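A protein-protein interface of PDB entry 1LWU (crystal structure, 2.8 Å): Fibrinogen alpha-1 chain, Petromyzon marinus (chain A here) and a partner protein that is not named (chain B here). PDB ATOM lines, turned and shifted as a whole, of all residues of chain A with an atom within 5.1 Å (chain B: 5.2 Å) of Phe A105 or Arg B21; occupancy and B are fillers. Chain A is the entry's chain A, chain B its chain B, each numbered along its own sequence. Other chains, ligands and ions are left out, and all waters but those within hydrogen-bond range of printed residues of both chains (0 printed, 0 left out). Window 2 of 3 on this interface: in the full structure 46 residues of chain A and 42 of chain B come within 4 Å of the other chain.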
ATOM      1  N   ILE A  38      -8.579  12.960  14.015  1.00  0.00           N
ATOM      2  CA  ILE A  38      -8.861  11.640  13.479  1.00  0.00           C
ATOM      3  C   ILE A  38     -10.175  11.165  14.062  1.00  0.00           C
ATOM      4  O   ILE A  38     -10.986  10.571  13.359  1.00  0.00           O
ATOM      5  CB  ILE A  38      -7.762  10.629  13.853  1.00  0.00           C
ATOM      6  CG1 ILE A  38      -6.441  11.030  13.189  1.00  0.00           C
ATOM      7  CG2 ILE A  38      -8.190   9.228  13.457  1.00  0.00           C
ATOM      8  CD1 ILE A  38      -6.573  11.395  11.733  1.00  0.00           C
ATOM      9  N   ASN A  39     -10.384  11.423  15.349  1.00  0.00           N
ATOM     10  CA  ASN A  39     -11.631  11.029  15.983  1.00  0.00           C
ATOM     11  C   ASN A  39     -12.792  11.664  15.242  1.00  0.00           C
ATOM     12  O   ASN A  39     -13.744  10.979  14.871  1.00  0.00           O
ATOM     13  CB  ASN A  39     -11.667  11.455  17.441  1.00  0.00           C
ATOM     14  CG  ASN A  39     -10.710  10.662  18.290  1.00  0.00           C
ATOM     15  OD1 ASN A  39     -10.517   9.464  18.072  1.00  0.00           O
ATOM     16  ND2 ASN A  39     -10.104  11.321  19.276  1.00  0.00           N
ATOM     17  N   LEU A  42     -13.538   9.990  12.067  1.00  0.00           N
ATOM     18  CA  LEU A  42     -14.192   8.694  12.144  1.00  0.00           C
ATOM     19  C   LEU A  42     -15.616   8.880  12.648  1.00  0.00           C
ATOM     20  O   LEU A  42     -16.398   7.936  12.681  1.00  0.00           O
ATOM     21  CB  LEU A  42     -13.411   7.752  13.058  1.00  0.00           C
ATOM     22  CG  LEU A  42     -11.954   7.530  12.631  1.00  0.00           C
ATOM     23  CD1 LEU A  42     -11.288   6.552  13.574  1.00  0.00           C
ATOM     24  CD2 LEU A  42     -11.884   7.013  11.211  1.00  0.00           C
ATOM     25  N   ASN A 102     -13.789  -0.229  10.066  1.00  0.00           N
ATOM     26  CA  ASN A 102     -12.651   0.086  10.923  1.00  0.00           C
ATOM     27  C   ASN A 102     -12.856   1.498  11.474  1.00  0.00           C
ATOM     28  O   ASN A 102     -12.083   1.985  12.306  1.00  0.00           O
ATOM     29  CB  ASN A 102     -11.342   0.040  10.117  1.00  0.00           C
ATOM     30  CG  ASN A 102     -11.126  -1.292   9.405  1.00  0.00           C
ATOM     31  OD1 ASN A 102     -11.267  -2.362   9.999  1.00  0.00           O
ATOM     32  ND2 ASN A 102     -10.761  -1.227   8.129  1.00  0.00           N
ATOM     33  N   LEU A 103     -13.918   2.135  10.992  1.00  0.00           N
ATOM     34  CA  LEU A 103     -14.295   3.494  11.359  1.00  0.00           C
ATOM     35  C   LEU A 103     -14.561   3.710  12.839  1.00  0.00           C
ATOM     36  O   LEU A 103     -14.205   4.754  13.383  1.00  0.00           O
ATOM     37  CB  LEU A 103     -15.526   3.903  10.559  1.00  0.00           C
ATOM     38  CG  LEU A 103     -15.344   3.536   9.087  1.00  0.00           C
ATOM     39  CD1 LEU A 103     -16.583   3.935   8.296  1.00  0.00           C
ATOM     40  CD2 LEU A 103     -14.088   4.208   8.539  1.00  0.00           C
ATOM     41  N   LYS A 104     -15.200   2.740  13.486  1.00  0.00           N
ATOM     42  CA  LYS A 104     -15.490   2.859  14.912  1.00  0.00           C
ATOM     43  C   LYS A 104     -14.297   3.475  15.643  1.00  0.00           C
ATOM     44  O   LYS A 104     -14.435   4.502  16.313  1.00  0.00           O
ATOM     45  CB  LYS A 104     -15.795   1.485  15.529  1.00  0.00           C
ATOM     46  CG  LYS A 104     -17.257   1.052  15.504  1.00  0.00           C
ATOM     47  CD  LYS A 104     -17.436  -0.218  16.335  1.00  0.00           C
ATOM     48  CE  LYS A 104     -18.889  -0.647  16.435  1.00  0.00           C
ATOM     49  NZ  LYS A 104     -19.028  -1.875  17.271  1.00  0.00           N
ATOM     50  N   PHE A 105     -13.135   2.839  15.491  1.00  0.00           N
ATOM     51  CA  PHE A 105     -11.876   3.251  16.116  1.00  0.00           C
ATOM     52  C   PHE A 105     -11.875   4.618  16.811  1.00  0.00           C
ATOM     53  O   PHE A 105     -12.199   5.636  16.200  1.00  0.00           O
ATOM     54  CB  PHE A 105     -10.752   3.221  15.083  1.00  0.00           C
ATOM     55  CG  PHE A 105      -9.403   3.483  15.668  1.00  0.00           C
ATOM     56  CD1 PHE A 105      -8.844   2.589  16.580  1.00  0.00           C
ATOM     57  CD2 PHE A 105      -8.694   4.629  15.333  1.00  0.00           C
ATOM     58  CE1 PHE A 105      -7.595   2.829  17.151  1.00  0.00           C
ATOM     59  CE2 PHE A 105      -7.446   4.880  15.899  1.00  0.00           C
ATOM     60  CZ  PHE A 105      -6.896   3.975  16.810  1.00  0.00           C
ATOM     61  N   GLU A 106     -11.493   4.640  18.086  1.00  0.00           N
ATOM     62  CA  GLU A 106     -11.461   5.890  18.837  1.00  0.00           C
ATOM     63  C   GLU A 106     -10.761   5.763  20.194  1.00  0.00           C
ATOM     64  O   GLU A 106     -11.335   5.262  21.166  1.00  0.00           O
ATOM     65  CB  GLU A 106     -12.887   6.409  19.028  1.00  0.00           C
ATOM     66  CG  GLU A 106     -12.980   7.746  19.733  1.00  0.00           C
ATOM     67  CD  GLU A 106     -14.396   8.276  19.773  1.00  0.00           C
ATOM     68  OE1 GLU A 106     -14.978   8.484  18.685  1.00  0.00           O
ATOM     69  OE2 GLU A 106     -14.926   8.483  20.886  1.00  0.00           O
ATOM     70  N   ARG A 107      -9.515   6.231  20.235  1.00  0.00           N
ATOM     71  CA  ARG A 107      -8.674   6.213  21.432  1.00  0.00           C
ATOM     72  C   ARG A 107      -9.297   6.960  22.610  1.00  0.00           C
ATOM     73  O   ARG A 107     -10.470   7.332  22.566  1.00  0.00           O
ATOM     74  CB  ARG A 107      -7.317   6.827  21.105  1.00  0.00           C
ATOM     75  CG  ARG A 107      -7.418   8.133  20.324  1.00  0.00           C
ATOM     76  CD  ARG A 107      -7.938   7.927  18.896  1.00  0.00           C
ATOM     77  NE  ARG A 107      -6.865   7.732  17.924  1.00  0.00           N
ATOM     78  CZ  ARG A 107      -6.008   6.714  17.931  1.00  0.00           C
ATOM     79  NH1 ARG A 107      -6.088   5.775  18.863  1.00  0.00           N
ATOM     80  NH2 ARG A 107      -5.064   6.636  16.999  1.00  0.00           N
ATOM     81  N   GLU B  17       1.278   5.429  15.762  1.00  0.00           N
ATOM     82  CA  GLU B  17      -0.122   5.012  15.692  1.00  0.00           C
ATOM     83  C   GLU B  17      -1.090   5.984  15.000  1.00  0.00           C
ATOM     84  O   GLU B  17      -2.277   5.685  14.855  1.00  0.00           O
ATOM     85  CB  GLU B  17      -0.631   4.678  17.104  1.00  0.00           C
ATOM     86  CG  GLU B  17      -0.339   5.748  18.145  1.00  0.00           C
ATOM     87  CD  GLU B  17      -0.725   5.323  19.552  1.00  0.00           C
ATOM     88  OE1 GLU B  17      -1.928   5.106  19.805  1.00  0.00           O
ATOM     89  OE2 GLU B  17       0.178   5.207  20.407  1.00  0.00           O
ATOM     90  N   VAL B  18      -0.591   7.139  14.567  1.00  0.00           N
ATOM     91  CA  VAL B  18      -1.441   8.107  13.885  1.00  0.00           C
ATOM     92  C   VAL B  18      -1.243   7.992  12.379  1.00  0.00           C
ATOM     93  O   VAL B  18      -2.216   7.903  11.629  1.00  0.00           O
ATOM     94  CB  VAL B  18      -1.142   9.556  14.343  1.00  0.00           C
ATOM     95  CG1 VAL B  18      -1.940  10.548  13.520  1.00  0.00           C
ATOM     96  CG2 VAL B  18      -1.517   9.716  15.796  1.00  0.00           C
ATOM     97  N   LYS B  19       0.010   7.982  11.932  1.00  0.00           N
ATOM     98  CA  LYS B  19       0.296   7.861  10.503  1.00  0.00           C
ATOM     99  C   LYS B  19      -0.475   6.663   9.958  1.00  0.00           C
ATOM    100  O   LYS B  19      -0.834   6.619   8.781  1.00  0.00           O
ATOM    101  CB  LYS B  19       1.795   7.662  10.272  1.00  0.00           C
ATOM    102  CG  LYS B  19       2.247   7.969   8.851  1.00  0.00           C
ATOM    103  CD  LYS B  19       3.759   7.856   8.732  1.00  0.00           C
ATOM    104  CE  LYS B  19       4.301   8.553   7.479  1.00  0.00           C
ATOM    105  NZ  LYS B  19       3.873   7.932   6.191  1.00  0.00           N
ATOM    106  N   ILE B  20      -0.712   5.690  10.835  1.00  0.00           N
ATOM    107  CA  ILE B  20      -1.463   4.487  10.504  1.00  0.00           C
ATOM    108  C   ILE B  20      -2.851   4.942  10.082  1.00  0.00           C
ATOM    109  O   ILE B  20      -3.152   5.086   8.898  1.00  0.00           O
ATOM    110  CB  ILE B  20      -1.668   3.592  11.738  1.00  0.00           C
ATOM    111  CG1 ILE B  20      -0.335   3.284  12.404  1.00  0.00           C
ATOM    112  CG2 ILE B  20      -2.377   2.321  11.340  1.00  0.00           C
ATOM    113  CD1 ILE B  20      -0.479   2.425  13.658  1.00  0.00           C
ATOM    114  N   ARG B  21      -3.685   5.169  11.091  1.00  0.00           N
ATOM    115  CA  ARG B  21      -5.056   5.601  10.911  1.00  0.00           C
ATOM    116  C   ARG B  21      -5.229   6.582   9.770  1.00  0.00           C
ATOM    117  O   ARG B  21      -6.112   6.416   8.932  1.00  0.00           O
ATOM    118  CB  ARG B  21      -5.572   6.210  12.214  1.00  0.00           C
ATOM    119  CG  ARG B  21      -5.666   5.199  13.339  1.00  0.00           C
ATOM    120  CD  ARG B  21      -6.572   4.049  12.929  1.00  0.00           C
ATOM    121  NE  ARG B  21      -6.618   2.973  13.914  1.00  0.00           N
ATOM    122  CZ  ARG B  21      -7.381   1.888  13.803  1.00  0.00           C
ATOM    123  NH1 ARG B  21      -8.171   1.726  12.749  1.00  0.00           N
ATOM    124  NH2 ARG B  21      -7.359   0.964  14.755  1.00  0.00           N
ATOM    125  N   ILE B  22      -4.383   7.599   9.722  1.00  0.00           N
ATOM    126  CA  ILE B  22      -4.486   8.588   8.662  1.00  0.00           C
ATOM    127  C   ILE B  22      -4.208   8.035   7.264  1.00  0.00           C
ATOM    128  O   ILE B  22      -4.896   8.394   6.310  1.00  0.00           O
ATOM    129  CB  ILE B  22      -3.553   9.789   8.924  1.00  0.00           C
ATOM    130  CG1 ILE B  22      -4.065  10.569  10.139  1.00  0.00           C
ATOM    131  CG2 ILE B  22      -3.482  10.678   7.692  1.00  0.00           C
ATOM    132  CD1 ILE B  22      -3.423  11.931  10.333  1.00  0.00           C
ATOM    133  N   GLU B  23      -3.215   7.162   7.131  1.00  0.00           N
ATOM    134  CA  GLU B  23      -2.880   6.598   5.823  1.00  0.00           C
ATOM    135  C   GLU B  23      -3.744   5.409   5.397  1.00  0.00           C
ATOM    136  O   GLU B  23      -3.917   5.150   4.202  1.00  0.00           O
ATOM    137  CB  GLU B  23      -1.417   6.167   5.793  1.00  0.00           C
ATOM    138  CG  GLU B  23      -0.426   7.292   5.815  1.00  0.00           C
ATOM    139  CD  GLU B  23       0.978   6.792   5.588  1.00  0.00           C
ATOM    140  OE1 GLU B  23       1.428   5.931   6.374  1.00  0.00           O
ATOM    141  OE2 GLU B  23       1.625   7.258   4.625  1.00  0.00           O
ATOM    142  N   SER B  24      -4.272   4.676   6.370  1.00  0.00           N
ATOM    143  CA  SER B  24      -5.095   3.525   6.061  1.00  0.00           C
ATOM    144  C   SER B  24      -6.526   3.703   6.512  1.00  0.00           C
ATOM    145  O   SER B  24      -7.417   3.973   5.705  1.00  0.00           O
ATOM    146  CB  SER B  24      -4.517   2.273   6.713  1.00  0.00           C
ATOM    147  OG  SER B  24      -3.340   1.860   6.046  1.00  0.00           O
ATOM    148  N   THR B  25      -6.741   3.556   7.812  1.00  0.00           N
ATOM    149  CA  THR B  25      -8.070   3.666   8.386  1.00  0.00           C
ATOM    150  C   THR B  25      -8.926   4.818   7.857  1.00  0.00           C
ATOM    151  O   THR B  25     -10.148   4.738   7.902  1.00  0.00           O
ATOM    152  CB  THR B  25      -7.987   3.758   9.913  1.00  0.00           C
ATOM    153  OG1 THR B  25      -7.110   2.730  10.400  1.00  0.00           O
ATOM    154  CG2 THR B  25      -9.370   3.568  10.527  1.00  0.00           C
ATOM    155  N   VAL B  26      -8.305   5.882   7.357  1.00  0.00           N
ATOM    156  CA  VAL B  26      -9.079   7.004   6.827  1.00  0.00           C
ATOM    157  C   VAL B  26      -8.949   7.166   5.315  1.00  0.00           C
ATOM    158  O   VAL B  26      -9.942   7.061   4.595  1.00  0.00           O
ATOM    159  CB  VAL B  26      -8.720   8.353   7.522  1.00  0.00           C
ATOM    160  CG1 VAL B  26      -9.216   9.526   6.688  1.00  0.00           C
ATOM    161  CG2 VAL B  26      -9.384   8.422   8.893  1.00  0.00           C
ATOM    162  N   ALA B  27      -7.743   7.421   4.822  1.00  0.00           N
ATOM    163  CA  ALA B  27      -7.575   7.583   3.384  1.00  0.00           C
ATOM    164  C   ALA B  27      -8.069   6.326   2.655  1.00  0.00           C
ATOM    165  O   ALA B  27      -8.212   6.309   1.427  1.00  0.00           O
ATOM    166  CB  ALA B  27      -6.116   7.856   3.056  1.00  0.00           C
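O of Ile B22 is in hydrogen-bond range of N of Ala B27, 3.4 Å away.
The backbone carbonyl oxygen (O) of Arg B21 is in hydrogen-bond range of the backbone NH (N) of Val B26 (2.8 Å).
OG1 of Thr B25 is in hydrogen-bond range of NH1 of Arg B21 (2.8 Å).
Among the printed residues, pairs that only touch across the chains: Phe A105 with Arg B21 (2.9 Å), Ile A38 with Ile B22 (3.1 Å), Asn A102 with Thr B25 (3.6 Å), Arg A107 with Glu B17 (3.6 Å), Leu A42 with Val B26 (3.7 Å), Asn A102 with Arg B21 (3.9 Å) and Arg A107 with Arg B21 (3.98 Å).
Printed residues of chain B within 4 Å of Phe A105: Arg B21 (2.9 Å).
Arg B21 touches three residues of chain A.
Of the printed residues of chain A, Thr B25 touches Asn A102 (3.6 Å).
Of the printed residues of chain B, Asn A102 touches Arg B21 (3.9 Å) and Thr B25 (3.6 Å).
Printed residues of chain B within 4 Å of Ile A38: Ile B22 (3.1 Å).
Of the printed residues of chain A, Glu B17 touches Arg A107 (3.6 Å).
Of the printed residues of chain B, Arg A107 touches Glu B17 and Arg B21.
Ser B24 touches none of the printed residues of chain A.
The nearest residue of chain B that does not touch Phe A105 is Thr B25 (4.8 Å).
Of the 9 printed residues of chain A, 5 touch a printed residue of chain B.
Printed residues of chain A that touch a printed residue of chain B: Ile A38, Leu A42, Asn A102, Phe A105 and Arg A107.
Hydrophobic or aromatic side chains of chain A within 4 Å of the printed part of chain B: Ile A38, Leu A42 and Phe A105.
Printed residues of chain B that touch a printed residue of chain A: Glu B17, Arg B21, Ile B22, Thr B25 and Val B26.
Hydrophobic or aromatic side chains of chain B within 4 Å of the printed part of chain A: Ile B22 and Val B26.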
